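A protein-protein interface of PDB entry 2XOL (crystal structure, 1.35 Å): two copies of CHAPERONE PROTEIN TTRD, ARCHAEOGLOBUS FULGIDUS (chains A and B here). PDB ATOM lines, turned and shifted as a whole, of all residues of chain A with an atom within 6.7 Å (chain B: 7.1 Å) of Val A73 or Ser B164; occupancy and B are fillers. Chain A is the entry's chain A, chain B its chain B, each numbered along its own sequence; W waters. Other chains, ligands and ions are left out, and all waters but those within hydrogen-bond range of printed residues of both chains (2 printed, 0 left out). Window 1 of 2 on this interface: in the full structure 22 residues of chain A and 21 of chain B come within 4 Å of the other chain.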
ATOM      1  N   MET A  62      21.344  14.926 -11.843  1.00  0.00           N
ATOM      2  CA  MET A  62      20.348  15.972 -12.000  1.00  0.00           C
ATOM      3  C   MET A  62      19.036  15.367 -12.472  1.00  0.00           C
ATOM      4  O   MET A  62      18.882  15.067 -13.653  1.00  0.00           O
ATOM      5  CB  MET A  62      20.795  17.076 -12.951  1.00  0.00           C
ATOM      6  CG  MET A  62      19.908  18.299 -12.799  1.00  0.00           C
ATOM      7  SD  MET A  62      20.371  19.636 -13.880  1.00  0.00           S
ATOM      8  CE  MET A  62      21.968  20.082 -13.172  1.00  0.00           C
ATOM      9  N   GLU A  68      14.151  22.732 -15.377  1.00  0.00           N
ATOM     10  CA  GLU A  68      13.659  24.097 -15.550  1.00  0.00           C
ATOM     11  C   GLU A  68      14.427  25.104 -14.689  1.00  0.00           C
ATOM     12  O   GLU A  68      14.843  26.160 -15.180  1.00  0.00           O
ATOM     13  CB  GLU A  68      12.169  24.164 -15.229  1.00  0.00           C
ATOM     14  CG  GLU A  68      11.515  25.502 -15.524  1.00  0.00           C
ATOM     15  CD  GLU A  68      10.004  25.444 -15.350  1.00  0.00           C
ATOM     16  OE1 GLU A  68       9.451  26.355 -14.691  1.00  0.00           O
ATOM     17  OE2 GLU A  68       9.378  24.484 -15.867  1.00  0.00           O
ATOM     18  N   VAL A  69      14.628  24.789 -13.415  1.00  0.00           N
ATOM     19  CA  VAL A  69      15.390  25.702 -12.560  1.00  0.00           C
ATOM     20  C   VAL A  69      16.843  25.709 -13.037  1.00  0.00           C
ATOM     21  O   VAL A  69      17.493  26.731 -12.907  1.00  0.00           O
ATOM     22  CB  VAL A  69      15.321  25.397 -11.013  1.00  0.00           C
ATOM     23  CG1 VAL A  69      13.936  25.714 -10.417  1.00  0.00           C
ATOM     24  CG2 VAL A  69      15.745  23.990 -10.698  1.00  0.00           C
ATOM     25  N   TYR A  70      17.345  24.598 -13.588  1.00  0.00           N
ATOM     26  CA  TYR A  70      18.719  24.605 -14.086  1.00  0.00           C
ATOM     27  C   TYR A  70      18.864  25.590 -15.251  1.00  0.00           C
ATOM     28  O   TYR A  70      19.865  26.276 -15.361  1.00  0.00           O
ATOM     29  CB  TYR A  70      19.187  23.209 -14.496  1.00  0.00           C
ATOM     30  CG  TYR A  70      20.678  23.148 -14.782  1.00  0.00           C
ATOM     31  CD1 TYR A  70      21.608  23.447 -13.797  1.00  0.00           C
ATOM     32  CD2 TYR A  70      21.155  22.794 -16.037  1.00  0.00           C
ATOM     33  CE1 TYR A  70      22.966  23.403 -14.044  1.00  0.00           C
ATOM     34  CE2 TYR A  70      22.515  22.724 -16.284  1.00  0.00           C
ATOM     35  CZ  TYR A  70      23.421  23.024 -15.290  1.00  0.00           C
ATOM     36  OH  TYR A  70      24.767  22.949 -15.528  1.00  0.00           O
ATOM     37  N   GLU A  71      17.870  25.671 -16.128  1.00  0.00           N
ATOM     38  CA  GLU A  71      17.911  26.694 -17.171  1.00  0.00           C
ATOM     39  C   GLU A  71      18.033  28.094 -16.572  1.00  0.00           C
ATOM     40  O   GLU A  71      18.762  28.946 -17.104  1.00  0.00           O
ATOM     41  CB  GLU A  71      16.685  26.611 -18.088  1.00  0.00           C
ATOM     42  CG  GLU A  71      16.698  27.606 -19.247  1.00  0.00           C
ATOM     43  CD  GLU A  71      16.364  27.007 -20.633  1.00  0.00           C
ATOM     44  OE1 GLU A  71      15.847  25.875 -20.725  1.00  0.00           O
ATOM     45  OE2 GLU A  71      16.652  27.684 -21.656  1.00  0.00           O
ATOM     46  N   SER A  72      17.327  28.326 -15.459  1.00  0.00           N
ATOM     47  CA  SER A  72      17.428  29.609 -14.733  1.00  0.00           C
ATOM     48  C   SER A  72      18.847  29.856 -14.206  1.00  0.00           C
ATOM     49  O   SER A  72      19.340  30.985 -14.253  1.00  0.00           O
ATOM     50  CB  SER A  72      16.415  29.680 -13.551  1.00  0.00           C
ATOM     51  OG  SER A  72      15.110  29.729 -14.058  1.00  0.00           O
ATOM     52  N   VAL A  73      19.470  28.806 -13.686  1.00  0.00           N
ATOM     53  CA  VAL A  73      20.863  28.886 -13.226  1.00  0.00           C
ATOM     54  C   VAL A  73      21.781  29.330 -14.367  1.00  0.00           C
ATOM     55  O   VAL A  73      22.627  30.217 -14.209  1.00  0.00           O
ATOM     56  CB  VAL A  73      21.350  27.540 -12.666  1.00  0.00           C
ATOM     57  CG1 VAL A  73      22.838  27.546 -12.370  1.00  0.00           C
ATOM     58  CG2 VAL A  73      20.563  27.166 -11.395  1.00  0.00           C
ATOM     59  N   MET A  74      21.602  28.699 -15.530  1.00  0.00           N
ATOM     60  CA  MET A  74      22.438  29.002 -16.673  1.00  0.00           C
ATOM     61  C   MET A  74      22.235  30.454 -17.106  1.00  0.00           C
ATOM     62  O   MET A  74      23.186  31.182 -17.318  1.00  0.00           O
ATOM     63  CB  MET A  74      22.105  28.050 -17.840  1.00  0.00           C
ATOM     64  CG  MET A  74      22.366  26.581 -17.559  1.00  0.00           C
ATOM     65  SD  MET A  74      24.067  26.259 -17.017  1.00  0.00           S
ATOM     66  CE  MET A  74      25.002  26.912 -18.404  1.00  0.00           C
ATOM     67  N   LYS A  75      20.978  30.877 -17.246  1.00  0.00           N
ATOM     68  CA  LYS A  75      20.694  32.227 -17.671  1.00  0.00           C
ATOM     69  C   LYS A  75      21.209  33.277 -16.687  1.00  0.00           C
ATOM     70  O   LYS A  75      21.649  34.334 -17.100  1.00  0.00           O
ATOM     71  CB  LYS A  75      19.198  32.422 -17.937  1.00  0.00           C
ATOM     72  CG  LYS A  75      18.765  31.729 -19.215  1.00  0.00           C
ATOM     73  CD  LYS A  75      17.444  32.261 -19.718  1.00  0.00           C
ATOM     74  CE  LYS A  75      16.894  31.420 -20.865  1.00  0.00           C
ATOM     75  NZ  LYS A  75      15.585  31.958 -21.360  1.00  0.00           N
ATOM     76  N   ASP A  76      21.173  32.965 -15.392  1.00  0.00           N
ATOM     77  CA  ASP A  76      21.709  33.857 -14.368  1.00  0.00           C
ATOM     78  C   ASP A  76      23.236  34.049 -14.541  1.00  0.00           C
ATOM     79  O   ASP A  76      23.735  35.165 -14.459  1.00  0.00           O
ATOM     80  CB  ASP A  76      21.362  33.311 -12.980  1.00  0.00           C
ATOM     81  CG  ASP A  76      22.026  34.075 -11.865  1.00  0.00           C
ATOM     82  OD1 ASP A  76      21.657  35.244 -11.637  1.00  0.00           O
ATOM     83  OD2 ASP A  76      22.924  33.492 -11.226  1.00  0.00           O
ATOM     84  N   PHE A  77      23.957  32.966 -14.832  1.00  0.00           N
ATOM     85  CA  PHE A  77      25.407  33.029 -15.053  1.00  0.00           C
ATOM     86  C   PHE A  77      25.657  33.860 -16.318  1.00  0.00           C
ATOM     87  O   PHE A  77      26.456  34.791 -16.330  1.00  0.00           O
ATOM     88  CB  PHE A  77      25.981  31.611 -15.174  1.00  0.00           C
ATOM     89  CG  PHE A  77      27.460  31.482 -14.889  1.00  0.00           C
ATOM     90  CD1 PHE A  77      27.895  30.562 -13.958  1.00  0.00           C
ATOM     91  CD2 PHE A  77      28.397  32.253 -15.529  1.00  0.00           C
ATOM     92  CE1 PHE A  77      29.264  30.409 -13.690  1.00  0.00           C
ATOM     93  CE2 PHE A  77      29.753  32.115 -15.240  1.00  0.00           C
ATOM     94  CZ  PHE A  77      30.171  31.194 -14.324  1.00  0.00           C
ATOM     95  N   TYR A  78      24.932  33.541 -17.393  1.00  0.00           N
ATOM     96  CA  TYR A  78      25.110  34.246 -18.653  1.00  0.00           C
ATOM     97  C   TYR A  78      24.899  35.758 -18.506  1.00  0.00           C
ATOM     98  O   TYR A  78      25.683  36.561 -19.020  1.00  0.00           O
ATOM     99  CB  TYR A  78      24.140  33.707 -19.703  1.00  0.00           C
ATOM    100  CG  TYR A  78      24.374  32.272 -20.158  1.00  0.00           C
ATOM    101  CD1 TYR A  78      25.595  31.624 -20.007  1.00  0.00           C
ATOM    102  CD2 TYR A  78      23.361  31.588 -20.768  1.00  0.00           C
ATOM    103  CE1 TYR A  78      25.786  30.321 -20.456  1.00  0.00           C
ATOM    104  CE2 TYR A  78      23.528  30.295 -21.199  1.00  0.00           C
ATOM    105  CZ  TYR A  78      24.749  29.659 -21.055  1.00  0.00           C
ATOM    106  OH  TYR A  78      24.954  28.373 -21.502  1.00  0.00           O
ATOM    107  N   ARG A  80      25.192  37.800 -16.041  1.00  0.00           N
ATOM    108  CA  ARG A  80      26.257  38.474 -15.295  1.00  0.00           C
ATOM    109  C   ARG A  80      27.382  38.951 -16.207  1.00  0.00           C
ATOM    110  O   ARG A  80      28.163  39.841 -15.845  1.00  0.00           O
ATOM    111  CB  ARG A  80      26.913  37.482 -14.302  1.00  0.00           C
ATOM    112  CG  ARG A  80      26.180  37.055 -13.149  1.00  0.00           C
ATOM    113  CD  ARG A  80      27.212  36.714 -12.052  1.00  0.00           C
ATOM    114  NE  ARG A  80      27.644  35.317 -12.013  1.00  0.00           N
ATOM    115  CZ  ARG A  80      26.833  34.293 -11.729  1.00  0.00           C
ATOM    116  NH1 ARG A  80      25.526  34.480 -11.542  1.00  0.00           N
ATOM    117  NH2 ARG A  80      27.314  33.066 -11.648  1.00  0.00           N
ATOM    118  N   ALA A 132      31.627  24.370 -13.042  1.00  0.00           N
ATOM    119  CA  ALA A 132      30.252  24.277 -12.577  1.00  0.00           C
ATOM    120  C   ALA A 132      29.293  23.661 -13.619  1.00  0.00           C
ATOM    121  O   ALA A 132      28.373  22.934 -13.230  1.00  0.00           O
ATOM    122  CB  ALA A 132      29.752  25.648 -12.137  1.00  0.00           C
ATOM    123  N   HIS A 133      29.513  23.952 -14.910  1.00  0.00           N
ATOM    124  CA  HIS A 133      28.535  23.676 -15.961  1.00  0.00           C
ATOM    125  C   HIS A 133      29.085  22.885 -17.132  1.00  0.00           C
ATOM    126  O   HIS A 133      28.513  21.845 -17.470  1.00  0.00           O
ATOM    127  CB  HIS A 133      27.882  24.973 -16.408  1.00  0.00           C
ATOM    128  CG  HIS A 133      27.220  25.686 -15.287  1.00  0.00           C
ATOM    129  ND1 HIS A 133      26.170  25.132 -14.600  1.00  0.00           N
ATOM    130  CD2 HIS A 133      27.510  26.859 -14.678  1.00  0.00           C
ATOM    131  CE1 HIS A 133      25.816  25.960 -13.627  1.00  0.00           C
ATOM    132  NE2 HIS A 133      26.604  27.015 -13.659  1.00  0.00           N
ATOM    133  N   MET B   3      15.772  37.833 -12.275  1.00  0.00           N
ATOM    134  CA  MET B   3      15.449  36.639 -11.515  1.00  0.00           C
ATOM    135  C   MET B   3      16.088  36.732 -10.109  1.00  0.00           C
ATOM    136  O   MET B   3      15.391  36.565  -9.106  1.00  0.00           O
ATOM    137  CB  MET B   3      15.880  35.393 -12.289  1.00  0.00           C
ATOM    138  CG  MET B   3      15.439  34.095 -11.665  1.00  0.00           C
ATOM    139  SD  MET B   3      16.501  33.574 -10.301  1.00  0.00           S
ATOM    140  CE  MET B   3      18.027  33.250 -11.167  1.00  0.00           C
ATOM    141  N   TYR B 120      30.196  32.145  -5.692  1.00  0.00           N
ATOM    142  CA  TYR B 120      30.016  30.705  -5.496  1.00  0.00           C
ATOM    143  C   TYR B 120      29.908  30.370  -3.997  1.00  0.00           C
ATOM    144  O   TYR B 120      29.046  29.617  -3.580  1.00  0.00           O
ATOM    145  CB  TYR B 120      31.180  29.963  -6.194  1.00  0.00           C
ATOM    146  CG  TYR B 120      31.250  28.466  -6.056  1.00  0.00           C
ATOM    147  CD1 TYR B 120      30.153  27.664  -6.284  1.00  0.00           C
ATOM    148  CD2 TYR B 120      32.472  27.845  -5.844  1.00  0.00           C
ATOM    149  CE1 TYR B 120      30.232  26.300  -6.172  1.00  0.00           C
ATOM    150  CE2 TYR B 120      32.568  26.480  -5.754  1.00  0.00           C
ATOM    151  CZ  TYR B 120      31.445  25.708  -5.912  1.00  0.00           C
ATOM    152  OH  TYR B 120      31.519  24.334  -5.847  1.00  0.00           O
ATOM    153  N   ARG B 123      26.481  31.601  -2.746  1.00  0.00           N
ATOM    154  CA  ARG B 123      25.453  30.682  -3.196  1.00  0.00           C
ATOM    155  C   ARG B 123      25.473  29.345  -2.433  1.00  0.00           C
ATOM    156  O   ARG B 123      24.425  28.797  -2.096  1.00  0.00           O
ATOM    157  CB  ARG B 123      25.582  30.505  -4.718  1.00  0.00           C
ATOM    158  CG  ARG B 123      24.980  31.691  -5.471  1.00  0.00           C
ATOM    159  CD  ARG B 123      23.500  31.505  -5.653  1.00  0.00           C
ATOM    160  NE  ARG B 123      23.260  30.550  -6.727  1.00  0.00           N
ATOM    161  CZ  ARG B 123      23.222  30.818  -8.040  1.00  0.00           C
ATOM    162  NH1 ARG B 123      22.997  29.834  -8.887  1.00  0.00           N
ATOM    163  NH2 ARG B 123      23.384  32.042  -8.517  1.00  0.00           N
ATOM    164  N   ASP B 157      13.020  27.549  -4.501  1.00  0.00           N
ATOM    165  CA  ASP B 157      14.311  28.197  -4.332  1.00  0.00           C
ATOM    166  C   ASP B 157      15.383  27.162  -3.955  1.00  0.00           C
ATOM    167  O   ASP B 157      16.509  27.253  -4.438  1.00  0.00           O
ATOM    168  CB  ASP B 157      14.248  29.347  -3.317  1.00  0.00           C
ATOM    169  CG  ASP B 157      15.323  30.371  -3.570  1.00  0.00           C
ATOM    170  OD1 ASP B 157      15.431  30.869  -4.720  1.00  0.00           O
ATOM    171  OD2 ASP B 157      16.098  30.685  -2.626  1.00  0.00           O
ATOM    172  N   ALA B 158      15.034  26.184  -3.104  1.00  0.00           N
ATOM    173  CA  ALA B 158      15.935  25.090  -2.737  1.00  0.00           C
ATOM    174  C   ALA B 158      16.347  24.287  -3.976  1.00  0.00           C
ATOM    175  O   ALA B 158      17.516  23.923  -4.138  1.00  0.00           O
ATOM    176  CB  ALA B 158      15.300  24.172  -1.680  1.00  0.00           C
ATOM    177  N   LYS B 159      15.381  24.023  -4.835  1.00  0.00           N
ATOM    178  CA  LYS B 159      15.634  23.295  -6.090  1.00  0.00           C
ATOM    179  C   LYS B 159      16.584  24.061  -6.986  1.00  0.00           C
ATOM    180  O   LYS B 159      17.546  23.489  -7.499  1.00  0.00           O
ATOM    181  CB  LYS B 159      14.338  23.060  -6.837  1.00  0.00           C
ATOM    182  CG  LYS B 159      13.544  21.936  -6.257  1.00  0.00           C
ATOM    183  CD  LYS B 159      12.117  21.973  -6.750  1.00  0.00           C
ATOM    184  CE  LYS B 159      12.021  21.722  -8.217  1.00  0.00           C
ATOM    185  NZ  LYS B 159      10.591  21.726  -8.643  1.00  0.00           N
ATOM    186  N   TYR B 160      16.340  25.361  -7.144  1.00  0.00           N
ATOM    187  CA  TYR B 160      17.223  26.243  -7.882  1.00  0.00           C
ATOM    188  C   TYR B 160      18.657  26.191  -7.332  1.00  0.00           C
ATOM    189  O   TYR B 160      19.630  25.984  -8.077  1.00  0.00           O
ATOM    190  CB  TYR B 160      16.656  27.677  -7.870  1.00  0.00           C
ATOM    191  CG  TYR B 160      17.611  28.749  -8.325  1.00  0.00           C
ATOM    192  CD1 TYR B 160      17.892  28.944  -9.651  1.00  0.00           C
ATOM    193  CD2 TYR B 160      18.276  29.563  -7.397  1.00  0.00           C
ATOM    194  CE1 TYR B 160      18.756  29.915 -10.062  1.00  0.00           C
ATOM    195  CE2 TYR B 160      19.138  30.531  -7.815  1.00  0.00           C
ATOM    196  CZ  TYR B 160      19.376  30.721  -9.142  1.00  0.00           C
ATOM    197  OH  TYR B 160      20.278  31.669  -9.525  1.00  0.00           O
ATOM    198  N   LEU B 161      18.803  26.328  -6.012  1.00  0.00           N
ATOM    199  CA  LEU B 161      20.127  26.362  -5.401  1.00  0.00           C
ATOM    200  C   LEU B 161      20.839  25.029  -5.561  1.00  0.00           C
ATOM    201  O   LEU B 161      22.023  24.989  -5.919  1.00  0.00           O
ATOM    202  CB  LEU B 161      20.035  26.774  -3.923  1.00  0.00           C
ATOM    203  CG  LEU B 161      19.660  28.242  -3.674  1.00  0.00           C
ATOM    204  CD1 LEU B 161      19.258  28.444  -2.203  1.00  0.00           C
ATOM    205  CD2 LEU B 161      20.804  29.159  -4.070  1.00  0.00           C
ATOM    206  N   TYR B 162      20.114  23.938  -5.342  1.00  0.00           N
ATOM    207  CA  TYR B 162      20.711  22.599  -5.454  1.00  0.00           C
ATOM    208  C   TYR B 162      21.134  22.288  -6.905  1.00  0.00           C
ATOM    209  O   TYR B 162      22.218  21.738  -7.161  1.00  0.00           O
ATOM    210  CB  TYR B 162      19.758  21.544  -4.947  1.00  0.00           C
ATOM    211  CG  TYR B 162      20.291  20.158  -5.049  1.00  0.00           C
ATOM    212  CD1 TYR B 162      21.390  19.753  -4.302  1.00  0.00           C
ATOM    213  CD2 TYR B 162      19.722  19.247  -5.927  1.00  0.00           C
ATOM    214  CE1 TYR B 162      21.881  18.451  -4.410  1.00  0.00           C
ATOM    215  CE2 TYR B 162      20.211  17.951  -6.039  1.00  0.00           C
ATOM    216  CZ  TYR B 162      21.279  17.566  -5.274  1.00  0.00           C
ATOM    217  OH  TYR B 162      21.770  16.283  -5.380  1.00  0.00           O
ATOM    218  N   SER B 163      20.291  22.694  -7.847  1.00  0.00           N
ATOM    219  CA  SER B 163      20.563  22.451  -9.271  1.00  0.00           C
ATOM    220  C   SER B 163      21.803  23.192  -9.720  1.00  0.00           C
ATOM    221  O   SER B 163      22.480  22.723 -10.648  1.00  0.00           O
ATOM    222  CB  SER B 163      19.373  22.847 -10.149  1.00  0.00           C
ATOM    223  OG  SER B 163      19.358  24.232 -10.459  1.00  0.00           O
ATOM    224  N   SER B 164      22.084  24.336  -9.069  1.00  0.00           N
ATOM    225  CA  SER B 164      23.266  25.160  -9.327  1.00  0.00           C
ATOM    226  C   SER B 164      24.558  24.435  -8.974  1.00  0.00           C
ATOM    227  O   SER B 164      25.616  24.724  -9.540  1.00  0.00           O
ATOM    228  CB  SER B 164      23.240  26.434  -8.459  1.00  0.00           C
ATOM    229  OG  SER B 164      22.031  27.149  -8.559  1.00  0.00           O
ATOM    230  N   LEU B 165      24.458  23.522  -8.004  1.00  0.00           N
ATOM    231  CA  LEU B 165      25.618  22.937  -7.330  1.00  0.00           C
ATOM    232  C   LEU B 165      25.867  21.455  -7.635  1.00  0.00           C
ATOM    233  O   LEU B 165      26.992  20.964  -7.483  1.00  0.00           O
ATOM    234  CB  LEU B 165      25.434  23.091  -5.796  1.00  0.00           C
ATOM    235  CG  LEU B 165      25.285  24.517  -5.297  1.00  0.00           C
ATOM    236  CD1 LEU B 165      24.959  24.525  -3.805  1.00  0.00           C
ATOM    237  CD2 LEU B 165      26.537  25.297  -5.559  1.00  0.00           C
ATOM    238  N   VAL B 166      24.834  20.755  -8.081  1.00  0.00           N
ATOM    239  CA  VAL B 166      24.864  19.307  -8.159  1.00  0.00           C
ATOM    240  C   VAL B 166      25.878  18.755  -9.169  1.00  0.00           C
ATOM    241  O   VAL B 166      26.497  17.741  -8.921  1.00  0.00           O
ATOM    242  CB  VAL B 166      23.426  18.725  -8.373  1.00  0.00           C
ATOM    243  CG1 VAL B 166      22.874  19.103  -9.742  1.00  0.00           C
ATOM    244  CG2 VAL B 166      23.427  17.219  -8.139  1.00  0.00           C
ATOM    245  N   GLY B 167      26.072  19.451 -10.284  1.00  0.00           N
ATOM    246  CA  GLY B 167      27.013  18.974 -11.284  1.00  0.00           C
ATOM    247  C   GLY B 167      28.472  18.901 -10.842  1.00  0.00           C
ATOM    248  O   GLY B 167      29.158  17.892 -11.012  1.00  0.00           O
ATOM    249  N   GLU B 168      28.949  19.981 -10.260  1.00  0.00           N
ATOM    250  CA  GLU B 168      30.322  20.047  -9.799  1.00  0.00           C
ATOM    251  C   GLU B 168      30.551  19.140  -8.589  1.00  0.00           C
ATOM    252  O   GLU B 168      31.636  18.595  -8.412  1.00  0.00           O
ATOM    253  CB  GLU B 168      30.649  21.485  -9.448  1.00  0.00           C
ATOM    254  CG  GLU B 168      32.108  21.725  -9.135  1.00  0.00           C
ATOM    255  CD  GLU B 168      32.435  23.187  -9.020  1.00  0.00           C
ATOM    256  OE1 GLU B 168      33.604  23.491  -8.718  1.00  0.00           O
ATOM    257  OE2 GLU B 168      31.543  24.039  -9.279  1.00  0.00           O
HETATM  258  O   HOH W   1      23.593  30.874 -11.683  1.00  0.00           O
HETATM  259  O   HOH W   2      27.668  22.581 -10.574  1.00  0.00           O
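Glu A68 touches none of the printed residues of chain B. Val A73 touches three residues of chain B. Printed residues of chain B within 4 Å of Asp A76: Met B3 (3.8 Å), Arg B123 (3.1 Å) and Tyr B160 (3.6 Å). Ala B158 touches none of the printed residues of chain A. Of the printed residues of chain A, Lys B159 touches Val A69 (3.7 Å). Of chain A, only Val A73 comes within 4 Å of Ser B164. Of the printed residues of chain A, Glu B168 touches Ala A132 (3.5 Å). The nearest residue of chain B that does not touch Val A73 is Arg B123 (4.2 Å).
Hydrophobic or aromatic side chains of chain A that line the printed part of chain B: Met A62, Val A69, Tyr A70, Val A73 and Ala A132. Of the 15 printed residues of chain B, 8 touch a printed residue of chain A. Printed residues of chain B that touch a printed residue of chain A: Met B3, Arg B123, Lys B159, Tyr B160, Ser B163, Ser B164, Val B166 and Glu B168. Among the printed residues, Asp or Glu carboxylates within 4 Å of a Lys or Arg side-chain nitrogen of the other chain: Asp A76 with Arg B123 (3.1 Å).
Water W1 lies within hydrogen-bond range of OD2 of Asp A76, O of Val A73 and NH1 of Arg B123. Water W2 lies within hydrogen-bond range of the backbone carbonyl oxygen of Ala A132 (2.8 Å), the backbone NH of Glu B168 (2.9 Å) and the backbone carbonyl oxygen of Ser B164 (3.1 Å).
OG of Ser B163 sits at hydrogen-bond distance from O of Tyr B160, 3.0 Å away. The side-chain hydroxyl (OG) of Ser B164 is in hydrogen-bond range of the backbone carbonyl oxygen (O) of Tyr B160 (2.7 Å). NH1 of Arg B123 sits at hydrogen-bond distance from OG of Ser B164 (2.9 Å). NH2 of Arg B123 sits at hydrogen-bond distance from OH of Tyr B160, 3.3 Å away. The side-chain carboxylate of Glu B168 lies within hydrogen-bond range of the side-chain hydroxyl of Tyr B120. The side-chain hydroxyl (OH) of Tyr A70 is in hydrogen-bond range of a ring nitrogen (ND1) of His A133 (2.8 Å).
The side-chain carboxylate (OD2) of Asp A76 is in salt-bridge range of the guanidinium group (NH2) of Arg B123 (3.1 Å).
No position is printed for both chains.
Among the printed residues, merely in contact across the chains: Met A62 with Ser B163, Met A62 with Val B166, Val A69 with Lys B159, Val A69 with Tyr B160, Val A69 with Ser B163, Tyr A70 with Ser B163, Val A73 with Tyr B160, Val A73 with Ser B163, Val A73 with Ser B164, Asp A76 with Met B3, Asp A76 with Tyr B160 and Ala A132 with Glu B168.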
